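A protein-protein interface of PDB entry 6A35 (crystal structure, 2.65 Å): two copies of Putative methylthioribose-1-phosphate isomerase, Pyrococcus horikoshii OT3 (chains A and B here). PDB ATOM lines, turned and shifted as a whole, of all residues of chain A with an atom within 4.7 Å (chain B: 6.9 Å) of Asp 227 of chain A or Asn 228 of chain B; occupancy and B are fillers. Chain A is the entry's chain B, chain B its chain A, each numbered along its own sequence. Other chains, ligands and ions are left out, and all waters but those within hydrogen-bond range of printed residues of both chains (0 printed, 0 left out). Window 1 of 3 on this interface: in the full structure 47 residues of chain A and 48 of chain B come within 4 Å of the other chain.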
ATOM      1  N   HIS A 166     -23.587  35.528   8.450  1.00  0.00           N
ATOM      2  CA  HIS A 166     -23.835  34.433   7.506  1.00  0.00           C
ATOM      3  C   HIS A 166     -25.211  34.546   6.846  1.00  0.00           C
ATOM      4  O   HIS A 166     -26.182  34.932   7.507  1.00  0.00           O
ATOM      5  CB  HIS A 166     -23.779  33.101   8.255  1.00  0.00           C
ATOM      6  CG  HIS A 166     -23.336  31.958   7.406  1.00  0.00           C
ATOM      7  ND1 HIS A 166     -22.206  32.021   6.625  1.00  0.00           N
ATOM      8  CD2 HIS A 166     -23.846  30.714   7.235  1.00  0.00           C
ATOM      9  CE1 HIS A 166     -22.050  30.871   5.990  1.00  0.00           C
ATOM     10  NE2 HIS A 166     -23.028  30.057   6.349  1.00  0.00           N
ATOM     11  N   ASP A 199     -19.977  36.422   4.735  1.00  0.00           N
ATOM     12  CA  ASP A 199     -19.883  35.145   4.019  1.00  0.00           C
ATOM     13  C   ASP A 199     -20.805  35.110   2.819  1.00  0.00           C
ATOM     14  O   ASP A 199     -22.005  35.134   2.971  1.00  0.00           O
ATOM     15  CB  ASP A 199     -20.327  33.992   4.912  1.00  0.00           C
ATOM     16  CG  ASP A 199     -19.387  33.735   6.046  1.00  0.00           C
ATOM     17  OD1 ASP A 199     -18.343  34.424   6.165  1.00  0.00           O
ATOM     18  OD2 ASP A 199     -19.701  32.815   6.823  1.00  0.00           O
ATOM     19  N   GLU A 200     -20.267  35.009   1.619  1.00  0.00           N
ATOM     20  CA  GLU A 200     -21.136  35.003   0.466  1.00  0.00           C
ATOM     21  C   GLU A 200     -22.274  33.974   0.647  1.00  0.00           C
ATOM     22  O   GLU A 200     -23.392  34.243   0.277  1.00  0.00           O
ATOM     23  CB  GLU A 200     -20.339  34.798  -0.841  1.00  0.00           C
ATOM     24  CG  GLU A 200     -19.888  33.378  -1.103  1.00  0.00           C
ATOM     25  CD  GLU A 200     -19.015  33.235  -2.335  1.00  0.00           C
ATOM     26  OE1 GLU A 200     -18.942  34.151  -3.171  1.00  0.00           O
ATOM     27  OE2 GLU A 200     -18.374  32.173  -2.473  1.00  0.00           O
ATOM     28  N   THR A 201     -21.968  32.822   1.236  1.00  0.00           N
ATOM     29  CA  THR A 201     -22.945  31.755   1.608  1.00  0.00           C
ATOM     30  C   THR A 201     -23.448  30.920   0.447  1.00  0.00           C
ATOM     31  O   THR A 201     -24.624  30.904   0.155  1.00  0.00           O
ATOM     32  CB  THR A 201     -24.176  32.284   2.382  1.00  0.00           C
ATOM     33  OG1 THR A 201     -23.789  33.374   3.238  1.00  0.00           O
ATOM     34  CG2 THR A 201     -24.855  31.139   3.193  1.00  0.00           C
ATOM     35  N   ARG A 202     -22.556  30.188  -0.205  1.00  0.00           N
ATOM     36  CA  ARG A 202     -22.990  29.135  -1.141  1.00  0.00           C
ATOM     37  C   ARG A 202     -23.907  28.120  -0.403  1.00  0.00           C
ATOM     38  O   ARG A 202     -23.813  28.013   0.822  1.00  0.00           O
ATOM     39  CB  ARG A 202     -21.753  28.442  -1.753  1.00  0.00           C
ATOM     40  CG  ARG A 202     -21.117  29.239  -2.849  1.00  0.00           C
ATOM     41  CD  ARG A 202     -21.942  29.180  -4.110  1.00  0.00           C
ATOM     42  NE  ARG A 202     -21.736  27.926  -4.828  1.00  0.00           N
ATOM     43  CZ  ARG A 202     -22.425  27.541  -5.903  1.00  0.00           C
ATOM     44  NH1 ARG A 202     -23.406  28.254  -6.395  1.00  0.00           N
ATOM     45  NH2 ARG A 202     -22.118  26.416  -6.490  1.00  0.00           N
ATOM     46  N   ILE A 225     -16.923  38.179   1.442  1.00  0.00           N
ATOM     47  CA  ILE A 225     -15.862  37.178   1.291  1.00  0.00           C
ATOM     48  C   ILE A 225     -16.422  35.815   0.960  1.00  0.00           C
ATOM     49  O   ILE A 225     -17.592  35.549   1.204  1.00  0.00           O
ATOM     50  CB  ILE A 225     -15.061  36.982   2.586  1.00  0.00           C
ATOM     51  CG1 ILE A 225     -15.965  36.621   3.758  1.00  0.00           C
ATOM     52  CG2 ILE A 225     -14.284  38.249   2.946  1.00  0.00           C
ATOM     53  CD1 ILE A 225     -15.261  36.006   4.917  1.00  0.00           C
ATOM     54  N   ALA A 226     -15.548  34.964   0.416  1.00  0.00           N
ATOM     55  CA  ALA A 226     -15.772  33.528   0.229  1.00  0.00           C
ATOM     56  C   ALA A 226     -15.902  32.795   1.561  1.00  0.00           C
ATOM     57  O   ALA A 226     -15.171  33.072   2.497  1.00  0.00           O
ATOM     58  CB  ALA A 226     -14.590  32.976  -0.524  1.00  0.00           C
ATOM     59  N   ASP A 227     -16.790  31.819   1.640  1.00  0.00           N
ATOM     60  CA  ASP A 227     -17.049  31.127   2.919  1.00  0.00           C
ATOM     61  C   ASP A 227     -15.763  30.468   3.477  1.00  0.00           C
ATOM     62  O   ASP A 227     -15.560  30.352   4.718  1.00  0.00           O
ATOM     63  CB  ASP A 227     -18.115  30.011   2.734  1.00  0.00           C
ATOM     64  CG  ASP A 227     -19.397  30.491   2.060  1.00  0.00           C
ATOM     65  OD1 ASP A 227     -19.972  31.464   2.544  1.00  0.00           O
ATOM     66  OD2 ASP A 227     -19.839  29.877   1.061  1.00  0.00           O
ATOM     67  N   ASN A 228     -14.943  29.987   2.530  1.00  0.00           N
ATOM     68  CA  ASN A 228     -13.645  29.373   2.797  1.00  0.00           C
ATOM     69  C   ASN A 228     -12.711  30.296   3.564  1.00  0.00           C
ATOM     70  O   ASN A 228     -11.826  29.792   4.254  1.00  0.00           O
ATOM     71  CB  ASN A 228     -12.927  29.054   1.465  1.00  0.00           C
ATOM     72  CG  ASN A 228     -13.181  27.644   0.939  1.00  0.00           C
ATOM     73  OD1 ASN A 228     -13.233  26.649   1.694  1.00  0.00           O
ATOM     74  ND2 ASN A 228     -13.261  27.546  -0.381  1.00  0.00           N
ATOM     75  N   ALA A 229     -12.864  31.619   3.393  1.00  0.00           N
ATOM     76  CA  ALA A 229     -12.016  32.628   4.041  1.00  0.00           C
ATOM     77  C   ALA A 229     -12.430  33.005   5.466  1.00  0.00           C
ATOM     78  O   ALA A 229     -11.736  33.838   6.084  1.00  0.00           O
ATOM     79  CB  ALA A 229     -11.999  33.921   3.200  1.00  0.00           C
ATOM     80  N   ALA A 230     -13.564  32.502   5.973  1.00  0.00           N
ATOM     81  CA  ALA A 230     -14.001  32.936   7.299  1.00  0.00           C
ATOM     82  C   ALA A 230     -12.926  32.595   8.303  1.00  0.00           C
ATOM     83  O   ALA A 230     -12.456  33.442   9.070  1.00  0.00           O
ATOM     84  CB  ALA A 230     -15.329  32.284   7.706  1.00  0.00           C
ATOM     85  N   ILE A 259     -26.713  26.280   5.870  1.00  0.00           N
ATOM     86  CA  ILE A 259     -25.429  25.542   5.748  1.00  0.00           C
ATOM     87  C   ILE A 259     -24.149  26.432   5.805  1.00  0.00           C
ATOM     88  O   ILE A 259     -24.001  27.374   5.048  1.00  0.00           O
ATOM     89  CB  ILE A 259     -25.436  24.665   4.454  1.00  0.00           C
ATOM     90  CG1 ILE A 259     -24.203  23.732   4.421  1.00  0.00           C
ATOM     91  CG2 ILE A 259     -25.548  25.536   3.187  1.00  0.00           C
ATOM     92  CD1 ILE A 259     -24.299  22.454   5.239  1.00  0.00           C
ATOM     93  N   GLY A 260     -23.235  26.106   6.708  1.00  0.00           N
ATOM     94  CA  GLY A 260     -22.035  26.885   6.893  1.00  0.00           C
ATOM     95  C   GLY A 260     -21.927  27.429   8.304  1.00  0.00           C
ATOM     96  O   GLY A 260     -20.809  27.691   8.813  1.00  0.00           O
ATOM     97  N   MET A 263     -19.976  25.393  10.750  1.00  0.00           N
ATOM     98  CA  MET A 263     -18.572  25.633  10.396  1.00  0.00           C
ATOM     99  C   MET A 263     -18.086  26.863  11.140  1.00  0.00           C
ATOM    100  O   MET A 263     -17.071  26.813  11.840  1.00  0.00           O
ATOM    101  CB  MET A 263     -18.421  25.812   8.867  1.00  0.00           C
ATOM    102  CG  MET A 263     -17.022  26.181   8.331  1.00  0.00           C
ATOM    103  SD  MET A 263     -16.716  27.947   8.074  1.00  0.00           S
ATOM    104  CE  MET A 263     -17.795  28.232   6.675  1.00  0.00           C
ATOM    105  N   ASP A 324     -27.422  23.254   8.285  1.00  0.00           N
ATOM    106  CA  ASP A 324     -26.799  22.398   9.286  1.00  0.00           C
ATOM    107  C   ASP A 324     -27.418  22.657  10.664  1.00  0.00           C
ATOM    108  O   ASP A 324     -28.213  23.612  10.840  1.00  0.00           O
ATOM    109  CB  ASP A 324     -25.240  22.505   9.293  1.00  0.00           C
ATOM    110  CG  ASP A 324     -24.702  23.960   9.325  1.00  0.00           C
ATOM    111  OD1 ASP A 324     -25.406  24.805   9.943  1.00  0.00           O
ATOM    112  OD2 ASP A 324     -23.550  24.219   8.774  1.00  0.00           O
ATOM    113  N   GLU B 200     -16.143  22.243  -3.895  1.00  0.00           N
ATOM    114  CA  GLU B 200     -16.105  23.038  -5.089  1.00  0.00           C
ATOM    115  C   GLU B 200     -14.950  24.074  -5.009  1.00  0.00           C
ATOM    116  O   GLU B 200     -14.302  24.366  -5.998  1.00  0.00           O
ATOM    117  CB  GLU B 200     -17.457  23.694  -5.331  1.00  0.00           C
ATOM    118  CG  GLU B 200     -17.773  24.865  -4.424  1.00  0.00           C
ATOM    119  CD  GLU B 200     -19.115  25.522  -4.727  1.00  0.00           C
ATOM    120  OE1 GLU B 200     -20.079  24.827  -5.102  1.00  0.00           O
ATOM    121  OE2 GLU B 200     -19.216  26.755  -4.579  1.00  0.00           O
ATOM    122  N   ARG B 202     -14.449  27.745  -3.595  1.00  0.00           N
ATOM    123  CA  ARG B 202     -14.567  29.135  -4.038  1.00  0.00           C
ATOM    124  C   ARG B 202     -13.294  29.817  -3.600  1.00  0.00           C
ATOM    125  O   ARG B 202     -12.618  29.307  -2.718  1.00  0.00           O
ATOM    126  CB  ARG B 202     -15.807  29.839  -3.435  1.00  0.00           C
ATOM    127  CG  ARG B 202     -17.106  29.690  -4.244  1.00  0.00           C
ATOM    128  CD  ARG B 202     -17.208  30.585  -5.475  1.00  0.00           C
ATOM    129  NE  ARG B 202     -17.628  31.949  -5.132  1.00  0.00           N
ATOM    130  CZ  ARG B 202     -17.696  32.975  -5.986  1.00  0.00           C
ATOM    131  NH1 ARG B 202     -17.348  32.871  -7.265  1.00  0.00           N
ATOM    132  NH2 ARG B 202     -18.116  34.146  -5.541  1.00  0.00           N
ATOM    133  N   ILE B 225     -19.506  18.972  -3.084  1.00  0.00           N
ATOM    134  CA  ILE B 225     -20.249  19.763  -2.123  1.00  0.00           C
ATOM    135  C   ILE B 225     -19.824  21.213  -2.136  1.00  0.00           C
ATOM    136  O   ILE B 225     -18.744  21.527  -2.637  1.00  0.00           O
ATOM    137  CB  ILE B 225     -20.019  19.258  -0.680  1.00  0.00           C
ATOM    138  CG1 ILE B 225     -18.557  19.375  -0.281  1.00  0.00           C
ATOM    139  CG2 ILE B 225     -20.476  17.811  -0.543  1.00  0.00           C
ATOM    140  CD1 ILE B 225     -18.298  19.048   1.158  1.00  0.00           C
ATOM    141  N   ALA B 226     -20.638  22.071  -1.502  1.00  0.00           N
ATOM    142  CA  ALA B 226     -20.289  23.465  -1.220  1.00  0.00           C
ATOM    143  C   ALA B 226     -19.279  23.517  -0.087  1.00  0.00           C
ATOM    144  O   ALA B 226     -19.267  22.596   0.750  1.00  0.00           O
ATOM    145  CB  ALA B 226     -21.547  24.241  -0.826  1.00  0.00           C
ATOM    146  N   ASP B 227     -18.472  24.595  -0.009  1.00  0.00           N
ATOM    147  CA  ASP B 227     -17.384  24.658   0.998  1.00  0.00           C
ATOM    148  C   ASP B 227     -17.978  24.681   2.404  1.00  0.00           C
ATOM    149  O   ASP B 227     -17.503  23.951   3.287  1.00  0.00           O
ATOM    150  CB  ASP B 227     -16.438  25.878   0.820  1.00  0.00           C
ATOM    151  CG  ASP B 227     -15.800  25.966  -0.583  1.00  0.00           C
ATOM    152  OD1 ASP B 227     -15.401  24.906  -1.127  1.00  0.00           O
ATOM    153  OD2 ASP B 227     -15.682  27.105  -1.119  1.00  0.00           O
ATOM    154  N   ASN B 228     -19.015  25.522   2.590  1.00  0.00           N
ATOM    155  CA  ASN B 228     -19.829  25.595   3.823  1.00  0.00           C
ATOM    156  C   ASN B 228     -20.196  24.226   4.382  1.00  0.00           C
ATOM    157  O   ASN B 228     -20.374  24.100   5.610  1.00  0.00           O
ATOM    158  CB  ASN B 228     -21.170  26.275   3.543  1.00  0.00           C
ATOM    159  CG  ASN B 228     -21.131  27.798   3.654  1.00  0.00           C
ATOM    160  OD1 ASN B 228     -20.468  28.369   4.539  1.00  0.00           O
ATOM    161  ND2 ASN B 228     -21.896  28.467   2.783  1.00  0.00           N
ATOM    162  N   ALA B 229     -20.356  23.218   3.505  1.00  0.00           N
ATOM    163  CA  ALA B 229     -20.854  21.915   3.945  1.00  0.00           C
ATOM    164  C   ALA B 229     -19.807  20.958   4.482  1.00  0.00           C
ATOM    165  O   ALA B 229     -20.162  19.866   4.909  1.00  0.00           O
ATOM    166  CB  ALA B 229     -21.627  21.227   2.832  1.00  0.00           C
ATOM    167  N   ALA B 230     -18.530  21.331   4.437  1.00  0.00           N
ATOM    168  CA  ALA B 230     -17.473  20.392   4.792  1.00  0.00           C
ATOM    169  C   ALA B 230     -17.661  20.002   6.223  1.00  0.00           C
ATOM    170  O   ALA B 230     -17.610  18.831   6.569  1.00  0.00           O
ATOM    171  CB  ALA B 230     -16.100  21.019   4.596  1.00  0.00           C
ATOM    172  N   ALA B 231     -17.932  20.989   7.048  1.00  0.00           N
ATOM    173  CA  ALA B 231     -18.105  20.758   8.455  1.00  0.00           C
ATOM    174  C   ALA B 231     -19.250  19.784   8.679  1.00  0.00           C
ATOM    175  O   ALA B 231     -19.076  18.732   9.290  1.00  0.00           O
ATOM    176  CB  ALA B 231     -18.371  22.068   9.164  1.00  0.00           C
ATOM    177  N   PHE B 232     -20.422  20.108   8.157  1.00  0.00           N
ATOM    178  CA  PHE B 232     -21.530  19.204   8.327  1.00  0.00           C
ATOM    179  C   PHE B 232     -21.158  17.741   7.978  1.00  0.00           C
ATOM    180  O   PHE B 232     -21.379  16.840   8.769  1.00  0.00           O
ATOM    181  CB  PHE B 232     -22.759  19.684   7.554  1.00  0.00           C
ATOM    182  CG  PHE B 232     -24.032  19.027   8.004  1.00  0.00           C
ATOM    183  CD1 PHE B 232     -24.479  19.182   9.310  1.00  0.00           C
ATOM    184  CD2 PHE B 232     -24.763  18.222   7.137  1.00  0.00           C
ATOM    185  CE1 PHE B 232     -25.632  18.569   9.741  1.00  0.00           C
ATOM    186  CE2 PHE B 232     -25.920  17.613   7.558  1.00  0.00           C
ATOM    187  CZ  PHE B 232     -26.353  17.788   8.863  1.00  0.00           C
ATOM    188  N   VAL B 233     -20.549  17.476   6.841  1.00  0.00           N
ATOM    189  CA  VAL B 233     -20.370  16.073   6.488  1.00  0.00           C
ATOM    190  C   VAL B 233     -19.400  15.438   7.486  1.00  0.00           C
ATOM    191  O   VAL B 233     -19.428  14.243   7.708  1.00  0.00           O
ATOM    192  CB  VAL B 233     -19.962  15.837   5.005  1.00  0.00           C
ATOM    193  CG1 VAL B 233     -20.808  16.674   4.057  1.00  0.00           C
ATOM    194  CG2 VAL B 233     -18.497  16.125   4.762  1.00  0.00           C
ATOM    195  N   ILE B 259      -7.153  28.883  -0.313  1.00  0.00           N
ATOM    196  CA  ILE B 259      -8.030  29.346   0.773  1.00  0.00           C
ATOM    197  C   ILE B 259      -9.156  28.357   1.154  1.00  0.00           C
ATOM    198  O   ILE B 259      -9.842  27.821   0.309  1.00  0.00           O
ATOM    199  CB  ILE B 259      -8.606  30.736   0.394  1.00  0.00           C
ATOM    200  CG1 ILE B 259      -9.473  31.318   1.506  1.00  0.00           C
ATOM    201  CG2 ILE B 259      -9.439  30.668  -0.875  1.00  0.00           C
ATOM    202  CD1 ILE B 259      -8.740  32.172   2.492  1.00  0.00           C
ATOM    203  N   GLY B 260      -9.336  28.127   2.447  1.00  0.00           N
ATOM    204  CA  GLY B 260     -10.287  27.121   2.928  1.00  0.00           C
ATOM    205  C   GLY B 260      -9.641  25.845   3.449  1.00  0.00           C
ATOM    206  O   GLY B 260     -10.333  24.980   4.015  1.00  0.00           O
ATOM    207  N   MET B 263      -9.567  26.247   7.319  1.00  0.00           N
ATOM    208  CA  MET B 263     -10.931  25.898   7.753  1.00  0.00           C
ATOM    209  C   MET B 263     -11.011  24.386   8.008  1.00  0.00           C
ATOM    210  O   MET B 263     -11.361  23.920   9.106  1.00  0.00           O
ATOM    211  CB  MET B 263     -11.921  26.340   6.658  1.00  0.00           C
ATOM    212  CG  MET B 263     -13.380  26.390   7.057  1.00  0.00           C
ATOM    213  SD  MET B 263     -14.326  24.993   6.413  1.00  0.00           S
ATOM    214  CE  MET B 263     -14.379  25.319   4.655  1.00  0.00           C
ATOM    215  N   LEU B 267     -11.401  21.966  11.463  1.00  0.00           N
ATOM    216  CA  LEU B 267     -12.578  21.096  11.571  1.00  0.00           C
ATOM    217  C   LEU B 267     -12.196  19.638  11.668  1.00  0.00           C
ATOM    218  O   LEU B 267     -12.871  18.864  12.370  1.00  0.00           O
ATOM    219  CB  LEU B 267     -13.491  21.296  10.373  1.00  0.00           C
ATOM    220  CG  LEU B 267     -14.169  22.654  10.329  1.00  0.00           C
ATOM    221  CD1 LEU B 267     -14.777  22.791   8.951  1.00  0.00           C
ATOM    222  CD2 LEU B 267     -15.219  22.757  11.388  1.00  0.00           C
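His 166 of chain A touches Asn 228 of chain B (CE1 to OD1, 3.3 Å).
Thr 201 of chain A touches Asn 228 of chain B.
Asn 228 of chain A touches Met 263 of chain B.
CA of Ala 229 of chain A touches CD1 of Ile 259 of chain B, 3.7 Å away.
Ile 259 of chain A touches Ala 229 of chain B (CD1 to CA, 3.7 Å).
Gly 260 of chain A touches Asn 228 of chain B (CA to OD1, 3.2 Å).
OD1 of Asn 228 of chain B touches CE of Met 263 of chain A, 3.4 Å away.
Ala 231 of chain B touches Met 263 of chain A.
Met 263 of chain B touches Met 263 of chain A.
Phe 232 of chain B touches Asp 324 of chain A (CD1 to CB, 3.4 Å).
Of the 15 printed residues of chain A, 11 touch a printed residue of chain B.
Hydrophobic or aromatic side chains of chain A that line the printed part of chain B: His 166, Ala 229, Ile 259 and Met 263.
Printed residues of chain B that touch a printed residue of chain A: Glu 200, Arg 202, Asp 227, Asn 228, Ala 229, Ala 231, Phe 232, Ile 259, Gly 260 and Met 263.
Hydrophobic or aromatic side chains of chain B that line the printed part of chain A: Ala 229, Ala 231, Phe 232, Ile 259 and Met 263.
The guanidinium group (NE) of Arg 202 of chain A lies within salt-bridge range of the side-chain carboxylate (OE2) of Glu 200 of chain B (2.8 Å).
OE1 of Glu 200 of chain A lies within salt-bridge range of NH2 of Arg 202 of chain B (2.5 Å).
The backbone carbonyl oxygen of Arg 202 of chain B lies within hydrogen-bond range of the side-chain amide nitrogen of Asn 228 of chain A, 3.0 Å away.
OD2 of Asp 227 of chain B sits at hydrogen-bond distance from ND2 of Asn 228 of chain A (2.6 Å).
The backbone carbonyl oxygen of Arg 202 of chain A lies within hydrogen-bond range of the side-chain amide nitrogen of Asn 228 of chain B (2.8 Å).
The side-chain carboxylate of Asp 227 of chain A sits at hydrogen-bond distance from the side-chain amide nitrogen of Asn 228 of chain B, 3.0 Å away.
The backbone carbonyl oxygen (O) of Ile 259 of chain A sits close to the side-chain amide nitrogen (ND2) of Asn 228 of chain B (3.3 Å).
ND2 of Asn 228 of chain A lies close to O of Ile 259 of chain B (3.5 Å).
The backbone carbonyl oxygen of Asn 228 of chain A sits close to the backbone NH of Gly 260 of chain B, at 3.5 Å.
Asp 227 of chain A touches just one residue of chain B: Asn 228.
Of chain A, only His 166, Thr 201, Arg 202, Asp 227, Ile 259, Gly 260 and Met 263 come within 4 Å of Asn 228 of chain B.
Of the printed residues of chain B, His 166 of chain A touches Asn 228.
Printed residues of chain A within 4 Å of Glu 200 of chain B: Arg 202 (2.8 Å).
Printed residues of chain B within 4 Å of Asp 324 of chain A: Phe 232.
Of the printed residues of chain B, Ile 259 of chain A touches Asn 228, Ala 229 and Phe 232.
Ala 230 of chain A touches none of the printed residues of chain B.
The nearest residue of chain B that does not touch Asp 227 of chain A is Asp 227 of chain B (4.9 Å).
The nearest residue of chain A that does not touch Asn 228 of chain B is Asp 324 of chain A (4.5 Å).
The nearest printed residue of chain B that does not touch Gly 260 of chain A is Ala 229 of chain B (5.2 Å).
Glu 200 of chain A touches Arg 202 of chain B, and with the chains exchanged Arg 202 of chain A touches Glu 200 of chain B.
Arg 202 of chain A touches Asn 228 of chain B, and with the chains exchanged Asn 228 of chain A touches Arg 202 of chain B.
Asp 227 of chain A touches Asn 228 of chain B, and with the chains exchanged Asn 228 of chain A touches Asp 227 of chain B.
Asn 228 of chain A touches Gly 260 of chain B, and with the chains exchanged Gly 260 of chain A touches Asn 228 of chain B.
11 positions are printed for both chains.
N of Arg 202 of chain B lies within hydrogen-bond range of OD2 of Asp 227 of chain B, 2.8 Å away.
A ring nitrogen (ND1) of His 166 of chain A lies within hydrogen-bond range of the side-chain carboxylate (OD2) of Asp 199 of chain A, at 2.6 Å.
O of Asp 199 of chain A is in hydrogen-bond range of OG1 of Thr 201 of chain A, 2.5 Å away.
The backbone NH of Glu 200 of chain A lies within hydrogen-bond range of the backbone carbonyl oxygen of Ile 225 of chain A (2.8 Å).
The side-chain carboxylate of Asp 227 of chain A is in hydrogen-bond range of the backbone NH of Arg 202 of chain A.
N of Gly 260 of chain A sits at hydrogen-bond distance from OD2 of Asp 324 of chain A.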
